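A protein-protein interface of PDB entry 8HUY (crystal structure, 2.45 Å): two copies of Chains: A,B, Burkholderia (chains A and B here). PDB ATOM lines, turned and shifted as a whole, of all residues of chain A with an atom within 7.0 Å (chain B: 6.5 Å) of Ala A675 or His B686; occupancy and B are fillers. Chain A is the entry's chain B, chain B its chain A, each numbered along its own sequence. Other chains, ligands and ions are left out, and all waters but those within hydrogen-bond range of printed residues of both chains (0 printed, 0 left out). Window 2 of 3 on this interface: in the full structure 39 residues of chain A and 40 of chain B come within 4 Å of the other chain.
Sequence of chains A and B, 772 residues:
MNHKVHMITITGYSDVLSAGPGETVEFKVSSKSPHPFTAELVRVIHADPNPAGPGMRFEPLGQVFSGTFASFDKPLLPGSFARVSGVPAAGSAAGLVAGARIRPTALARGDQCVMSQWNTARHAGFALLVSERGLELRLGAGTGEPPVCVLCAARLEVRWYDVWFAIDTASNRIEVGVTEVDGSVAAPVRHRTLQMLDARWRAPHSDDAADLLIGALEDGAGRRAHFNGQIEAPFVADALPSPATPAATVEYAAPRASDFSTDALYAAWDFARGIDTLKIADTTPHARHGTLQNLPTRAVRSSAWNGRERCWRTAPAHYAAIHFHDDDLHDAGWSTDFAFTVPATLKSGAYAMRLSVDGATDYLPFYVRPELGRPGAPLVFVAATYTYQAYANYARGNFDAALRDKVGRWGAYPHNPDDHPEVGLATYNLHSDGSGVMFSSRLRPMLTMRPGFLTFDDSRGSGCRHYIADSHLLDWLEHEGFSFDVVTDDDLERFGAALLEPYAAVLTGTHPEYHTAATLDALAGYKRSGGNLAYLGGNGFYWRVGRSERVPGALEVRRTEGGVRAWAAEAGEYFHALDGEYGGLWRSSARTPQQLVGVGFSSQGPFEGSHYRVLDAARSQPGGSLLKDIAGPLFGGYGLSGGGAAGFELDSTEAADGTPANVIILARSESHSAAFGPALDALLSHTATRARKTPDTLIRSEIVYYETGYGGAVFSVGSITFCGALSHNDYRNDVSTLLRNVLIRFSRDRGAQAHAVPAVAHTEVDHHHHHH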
ATOM      1  N   VAL A 564     -17.115  31.517  -5.318  1.00  0.00           N
ATOM      2  CA  VAL A 564     -16.991  31.624  -6.769  1.00  0.00           C
ATOM      3  C   VAL A 564     -18.393  31.884  -7.311  1.00  0.00           C
ATOM      4  O   VAL A 564     -19.252  31.002  -7.276  1.00  0.00           O
ATOM      5  CB  VAL A 564     -16.379  30.359  -7.379  1.00  0.00           C
ATOM      6  CG1 VAL A 564     -16.011  30.606  -8.838  1.00  0.00           C
ATOM      7  CG2 VAL A 564     -15.158  29.918  -6.592  1.00  0.00           C
ATOM      8  N   SER A 603     -11.362  23.742  -5.903  1.00  0.00           N
ATOM      9  CA  SER A 603     -10.707  24.309  -7.082  1.00  0.00           C
ATOM     10  C   SER A 603     -11.639  24.315  -8.295  1.00  0.00           C
ATOM     11  O   SER A 603     -12.440  23.398  -8.489  1.00  0.00           O
ATOM     12  CB  SER A 603      -9.425  23.551  -7.436  1.00  0.00           C
ATOM     13  OG  SER A 603      -8.851  24.090  -8.616  1.00  0.00           O
ATOM     14  N   GLN A 604     -11.508  25.352  -9.115  1.00  0.00           N
ATOM     15  CA  GLN A 604     -12.294  25.535 -10.325  1.00  0.00           C
ATOM     16  C   GLN A 604     -11.368  25.889 -11.479  1.00  0.00           C
ATOM     17  O   GLN A 604     -10.458  26.708 -11.320  1.00  0.00           O
ATOM     18  CB  GLN A 604     -13.334  26.645 -10.112  1.00  0.00           C
ATOM     19  CG  GLN A 604     -13.997  27.134 -11.373  1.00  0.00           C
ATOM     20  CD  GLN A 604     -13.638  28.574 -11.677  1.00  0.00           C
ATOM     21  OE1 GLN A 604     -13.614  29.426 -10.779  1.00  0.00           O
ATOM     22  NE2 GLN A 604     -13.336  28.854 -12.951  1.00  0.00           N
ATOM     23  N   GLY A 605     -11.588  25.275 -12.634  1.00  0.00           N
ATOM     24  CA  GLY A 605     -10.830  25.614 -13.812  1.00  0.00           C
ATOM     25  C   GLY A 605     -11.674  25.534 -15.068  1.00  0.00           C
ATOM     26  O   GLY A 605     -12.907  25.466 -15.015  1.00  0.00           O
ATOM     27  N   PRO A 606     -11.029  25.515 -16.226  1.00  0.00           N
ATOM     28  CA  PRO A 606     -11.776  25.353 -17.477  1.00  0.00           C
ATOM     29  C   PRO A 606     -12.257  23.915 -17.625  1.00  0.00           C
ATOM     30  O   PRO A 606     -11.948  23.037 -16.811  1.00  0.00           O
ATOM     31  CB  PRO A 606     -10.764  25.739 -18.561  1.00  0.00           C
ATOM     32  CG  PRO A 606      -9.652  26.455 -17.815  1.00  0.00           C
ATOM     33  CD  PRO A 606      -9.606  25.813 -16.463  1.00  0.00           C
ATOM     34  N   GLU A 608     -11.717  20.927 -18.472  1.00  0.00           N
ATOM     35  CA  GLU A 608     -10.585  20.060 -18.786  1.00  0.00           C
ATOM     36  C   GLU A 608     -10.405  19.051 -17.665  1.00  0.00           C
ATOM     37  O   GLU A 608     -10.531  19.392 -16.488  1.00  0.00           O
ATOM     38  CB  GLU A 608      -9.266  20.836 -18.965  1.00  0.00           C
ATOM     39  CG  GLU A 608      -9.376  22.242 -19.533  1.00  0.00           C
ATOM     40  CD  GLU A 608      -8.086  23.008 -19.376  1.00  0.00           C
ATOM     41  OE1 GLU A 608      -8.007  24.158 -19.835  1.00  0.00           O
ATOM     42  OE2 GLU A 608      -7.142  22.455 -18.778  1.00  0.00           O
ATOM     43  N   HIS A 672      -3.228  19.284 -13.212  1.00  0.00           N
ATOM     44  CA  HIS A 672      -4.188  20.138 -13.892  1.00  0.00           C
ATOM     45  C   HIS A 672      -3.481  21.344 -14.489  1.00  0.00           C
ATOM     46  O   HIS A 672      -2.408  21.752 -14.037  1.00  0.00           O
ATOM     47  CB  HIS A 672      -5.289  20.592 -12.942  1.00  0.00           C
ATOM     48  CG  HIS A 672      -5.947  19.466 -12.219  1.00  0.00           C
ATOM     49  ND1 HIS A 672      -6.950  18.711 -12.784  1.00  0.00           N
ATOM     50  CD2 HIS A 672      -5.734  18.952 -10.984  1.00  0.00           C
ATOM     51  CE1 HIS A 672      -7.337  17.785 -11.926  1.00  0.00           C
ATOM     52  NE2 HIS A 672      -6.618  17.911 -10.823  1.00  0.00           N
ATOM     53  N   SER A 673      -4.123  21.943 -15.492  1.00  0.00           N
ATOM     54  CA  SER A 673      -3.535  23.083 -16.173  1.00  0.00           C
ATOM     55  C   SER A 673      -3.399  24.273 -15.222  1.00  0.00           C
ATOM     56  O   SER A 673      -3.995  24.326 -14.134  1.00  0.00           O
ATOM     57  CB  SER A 673      -4.374  23.467 -17.388  1.00  0.00           C
ATOM     58  OG  SER A 673      -5.523  24.209 -17.002  1.00  0.00           O
ATOM     59  N   ALA A 674      -2.573  25.236 -15.643  1.00  0.00           N
ATOM     60  CA  ALA A 674      -2.331  26.411 -14.822  1.00  0.00           C
ATOM     61  C   ALA A 674      -3.569  27.284 -14.685  1.00  0.00           C
ATOM     62  O   ALA A 674      -3.663  28.047 -13.722  1.00  0.00           O
ATOM     63  CB  ALA A 674      -1.176  27.228 -15.409  1.00  0.00           C
ATOM     64  N   ALA A 675      -4.529  27.170 -15.605  1.00  0.00           N
ATOM     65  CA  ALA A 675      -5.740  27.982 -15.549  1.00  0.00           C
ATOM     66  C   ALA A 675      -6.612  27.654 -14.344  1.00  0.00           C
ATOM     67  O   ALA A 675      -7.562  28.407 -14.061  1.00  0.00           O
ATOM     68  CB  ALA A 675      -6.551  27.804 -16.833  1.00  0.00           C
ATOM     69  N   PHE A 676      -6.315  26.547 -13.652  1.00  0.00           N
ATOM     70  CA  PHE A 676      -7.047  26.138 -12.463  1.00  0.00           C
ATOM     71  C   PHE A 676      -6.634  26.941 -11.238  1.00  0.00           C
ATOM     72  O   PHE A 676      -5.446  27.135 -10.966  1.00  0.00           O
ATOM     73  CB  PHE A 676      -6.827  24.656 -12.192  1.00  0.00           C
ATOM     74  CG  PHE A 676      -7.749  23.762 -12.962  1.00  0.00           C
ATOM     75  CD1 PHE A 676      -7.544  23.530 -14.312  1.00  0.00           C
ATOM     76  CD2 PHE A 676      -8.823  23.153 -12.334  1.00  0.00           C
ATOM     77  CE1 PHE A 676      -8.375  22.701 -15.016  1.00  0.00           C
ATOM     78  CE2 PHE A 676      -9.668  22.331 -13.035  1.00  0.00           C
ATOM     79  CZ  PHE A 676      -9.444  22.100 -14.383  1.00  0.00           C
ATOM     80  N   GLY A 677      -7.627  27.340 -10.457  1.00  0.00           N
ATOM     81  CA  GLY A 677      -7.410  28.215  -9.337  1.00  0.00           C
ATOM     82  C   GLY A 677      -8.248  27.823  -8.141  1.00  0.00           C
ATOM     83  O   GLY A 677      -9.039  26.864  -8.178  1.00  0.00           O
ATOM     84  N   PRO A 678      -8.047  28.540  -7.037  1.00  0.00           N
ATOM     85  CA  PRO A 678      -8.709  28.193  -5.781  1.00  0.00           C
ATOM     86  C   PRO A 678     -10.115  28.771  -5.637  1.00  0.00           C
ATOM     87  O   PRO A 678     -10.447  29.833  -6.162  1.00  0.00           O
ATOM     88  CB  PRO A 678      -7.769  28.780  -4.723  1.00  0.00           C
ATOM     89  CG  PRO A 678      -7.035  29.876  -5.426  1.00  0.00           C
ATOM     90  CD  PRO A 678      -6.916  29.464  -6.849  1.00  0.00           C
ATOM     91  N   ALA A 679     -10.947  28.025  -4.913  1.00  0.00           N
ATOM     92  CA  ALA A 679     -12.276  28.472  -4.521  1.00  0.00           C
ATOM     93  C   ALA A 679     -12.180  29.629  -3.533  1.00  0.00           C
ATOM     94  O   ALA A 679     -11.712  29.446  -2.404  1.00  0.00           O
ATOM     95  CB  ALA A 679     -13.037  27.300  -3.900  1.00  0.00           C
ATOM     96  N   LEU A 680     -12.710  30.795  -3.923  1.00  0.00           N
ATOM     97  CA  LEU A 680     -12.512  32.015  -3.137  1.00  0.00           C
ATOM     98  C   LEU A 680     -12.939  31.849  -1.691  1.00  0.00           C
ATOM     99  O   LEU A 680     -12.266  32.348  -0.780  1.00  0.00           O
ATOM    100  CB  LEU A 680     -13.275  33.175  -3.755  1.00  0.00           C
ATOM    101  CG  LEU A 680     -12.780  33.625  -5.121  1.00  0.00           C
ATOM    102  CD1 LEU A 680     -13.494  34.928  -5.552  1.00  0.00           C
ATOM    103  CD2 LEU A 680     -11.260  33.789  -5.109  1.00  0.00           C
ATOM    104  N   LEU A 683     -10.534  30.900   1.092  1.00  0.00           N
ATOM    105  CA  LEU A 683      -9.352  31.754   1.238  1.00  0.00           C
ATOM    106  C   LEU A 683      -9.537  32.807   2.326  1.00  0.00           C
ATOM    107  O   LEU A 683     -10.547  33.522   2.344  1.00  0.00           O
ATOM    108  CB  LEU A 683      -9.019  32.466  -0.077  1.00  0.00           C
ATOM    109  CG  LEU A 683      -8.660  31.593  -1.283  1.00  0.00           C
ATOM    110  CD1 LEU A 683      -8.216  32.430  -2.493  1.00  0.00           C
ATOM    111  CD2 LEU A 683      -7.612  30.560  -0.910  1.00  0.00           C
ATOM    112  N   ILE A 699      -5.757  22.679  -5.212  1.00  0.00           N
ATOM    113  CA  ILE A 699      -5.901  22.262  -6.602  1.00  0.00           C
ATOM    114  C   ILE A 699      -5.819  20.750  -6.708  1.00  0.00           C
ATOM    115  O   ILE A 699      -4.807  20.212  -7.169  1.00  0.00           O
ATOM    116  CB  ILE A 699      -4.830  22.908  -7.499  1.00  0.00           C
ATOM    117  CG1 ILE A 699      -4.724  24.408  -7.230  1.00  0.00           C
ATOM    118  CG2 ILE A 699      -5.149  22.649  -8.948  1.00  0.00           C
ATOM    119  CD1 ILE A 699      -5.984  25.185  -7.573  1.00  0.00           C
ATOM    120  N   PRO B 678      -4.357  40.035  -5.401  1.00  0.00           N
ATOM    121  CA  PRO B 678      -5.574  40.847  -5.341  1.00  0.00           C
ATOM    122  C   PRO B 678      -6.341  40.735  -4.035  1.00  0.00           C
ATOM    123  O   PRO B 678      -6.441  39.676  -3.423  1.00  0.00           O
ATOM    124  CB  PRO B 678      -6.404  40.293  -6.506  1.00  0.00           C
ATOM    125  CG  PRO B 678      -5.902  38.918  -6.724  1.00  0.00           C
ATOM    126  CD  PRO B 678      -4.470  38.916  -6.351  1.00  0.00           C
ATOM    127  N   LEU B 683     -13.019  40.317  -5.879  1.00  0.00           N
ATOM    128  CA  LEU B 683     -13.042  39.218  -6.840  1.00  0.00           C
ATOM    129  C   LEU B 683     -14.397  38.521  -6.860  1.00  0.00           C
ATOM    130  O   LEU B 683     -14.963  38.209  -5.802  1.00  0.00           O
ATOM    131  CB  LEU B 683     -11.954  38.183  -6.539  1.00  0.00           C
ATOM    132  CG  LEU B 683     -10.492  38.628  -6.660  1.00  0.00           C
ATOM    133  CD1 LEU B 683      -9.537  37.424  -6.593  1.00  0.00           C
ATOM    134  CD2 LEU B 683     -10.254  39.472  -7.919  1.00  0.00           C
ATOM    135  N   LEU B 684     -14.903  38.267  -8.077  1.00  0.00           N
ATOM    136  CA  LEU B 684     -15.976  37.304  -8.295  1.00  0.00           C
ATOM    137  C   LEU B 684     -15.453  35.880  -8.468  1.00  0.00           C
ATOM    138  O   LEU B 684     -16.157  34.920  -8.129  1.00  0.00           O
ATOM    139  CB  LEU B 684     -16.793  37.704  -9.522  1.00  0.00           C
ATOM    140  CG  LEU B 684     -17.626  38.964  -9.317  1.00  0.00           C
ATOM    141  CD1 LEU B 684     -18.348  39.359 -10.596  1.00  0.00           C
ATOM    142  CD2 LEU B 684     -18.613  38.756  -8.185  1.00  0.00           C
ATOM    143  N   SER B 685     -14.210  35.732  -8.920  1.00  0.00           N
ATOM    144  CA  SER B 685     -13.527  34.451  -9.037  1.00  0.00           C
ATOM    145  C   SER B 685     -12.028  34.730  -9.018  1.00  0.00           C
ATOM    146  O   SER B 685     -11.593  35.887  -8.973  1.00  0.00           O
ATOM    147  CB  SER B 685     -13.924  33.726 -10.318  1.00  0.00           C
ATOM    148  OG  SER B 685     -13.131  34.175 -11.407  1.00  0.00           O
ATOM    149  N   HIS B 686     -11.231  33.661  -9.087  1.00  0.00           N
ATOM    150  CA  HIS B 686      -9.789  33.870  -9.133  1.00  0.00           C
ATOM    151  C   HIS B 686      -9.318  34.429 -10.475  1.00  0.00           C
ATOM    152  O   HIS B 686      -8.149  34.827 -10.590  1.00  0.00           O
ATOM    153  CB  HIS B 686      -9.052  32.565  -8.784  1.00  0.00           C
ATOM    154  CG  HIS B 686      -8.881  31.627  -9.940  1.00  0.00           C
ATOM    155  ND1 HIS B 686      -9.904  30.823 -10.401  1.00  0.00           N
ATOM    156  CD2 HIS B 686      -7.801  31.348 -10.713  1.00  0.00           C
ATOM    157  CE1 HIS B 686      -9.466  30.102 -11.421  1.00  0.00           C
ATOM    158  NE2 HIS B 686      -8.192  30.399 -11.628  1.00  0.00           N
ATOM    159  N   THR B 687     -10.195  34.500 -11.479  1.00  0.00           N
ATOM    160  CA  THR B 687      -9.838  35.069 -12.770  1.00  0.00           C
ATOM    161  C   THR B 687     -10.681  36.283 -13.139  1.00  0.00           C
ATOM    162  O   THR B 687     -10.513  36.817 -14.236  1.00  0.00           O
ATOM    163  CB  THR B 687      -9.953  34.018 -13.883  1.00  0.00           C
ATOM    164  OG1 THR B 687     -11.252  33.412 -13.837  1.00  0.00           O
ATOM    165  CG2 THR B 687      -8.894  32.943 -13.725  1.00  0.00           C
ATOM    166  N   ALA B 688     -11.562  36.756 -12.257  1.00  0.00           N
ATOM    167  CA  ALA B 688     -12.411  37.884 -12.623  1.00  0.00           C
ATOM    168  C   ALA B 688     -12.709  38.791 -11.432  1.00  0.00           C
ATOM    169  O   ALA B 688     -13.133  38.323 -10.371  1.00  0.00           O
ATOM    170  CB  ALA B 688     -13.724  37.374 -13.233  1.00  0.00           C
ATOM    171  N   PRO B 695      -7.763  39.839 -12.565  1.00  0.00           N
ATOM    172  CA  PRO B 695      -7.318  40.349 -11.252  1.00  0.00           C
ATOM    173  C   PRO B 695      -6.014  41.133 -11.292  1.00  0.00           C
ATOM    174  O   PRO B 695      -5.817  42.032 -10.462  1.00  0.00           O
ATOM    175  CB  PRO B 695      -7.171  39.075 -10.409  1.00  0.00           C
ATOM    176  CG  PRO B 695      -7.238  37.925 -11.376  1.00  0.00           C
ATOM    177  CD  PRO B 695      -8.033  38.394 -12.544  1.00  0.00           C
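A ring nitrogen (NE2) of His B686 is in hydrogen-bond range of the backbone carbonyl oxygen of Ala A675 (3.2 Å).
A ring nitrogen (NE2) of His B686 lies close to the backbone NH (N) of Gly A677, at 3.3 Å.
Leu B684 touches Val A564 (O to CA, 3.7 Å).
O of Gln A604 touches CE1 of His B686, 3.5 Å away.
His B686 touches Phe A676 (NE2 to C, 3.8 Å).
CD1 of Leu A680 touches O of Leu B683 (3.6 Å).
C of Leu B684 touches CD1 of Leu A680 (3.6 Å).
Ser B685 touches Leu A680.
His B686 touches Leu A680.
Positions printed for both chains: 678 and 683.
Of the 17 printed residues of chain A, 6 touch a printed residue of chain B.
Hydrophobic or aromatic side chains of chain A that line the printed part of chain B: Leu A680.
Among the printed residues, 9 pairs touch across the chains.
OG of Ser B685 is in hydrogen-bond range of N of Thr B687 (3.0 Å).
N of Ala B688 lies within hydrogen-bond range of OG of Ser B685 (3.1 Å).
OG of Ser A603 is in hydrogen-bond range of O of Gly A677, at 2.8 Å.
The backbone NH (N) of Gly A677 is in hydrogen-bond range of the backbone carbonyl oxygen (O) of Gln A604 (3.0 Å).
The backbone NH (N) of Ala A675 sits close to the side-chain hydroxyl (OG) of Ser A673.
Ala A675 touches just one residue of chain B: His B686 (3.2 Å).
Printed residues of chain B within 4 Å of Phe A676: His B686.
Pro A678 touches none of the printed residues of chain B.
Of the printed residues of chain A, Leu B684 touches Val A564 and Leu A680.
Of the printed residues of chain A, His B686 touches Gln A604, Ala A675, Phe A676, Gly A677 and Leu A680.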
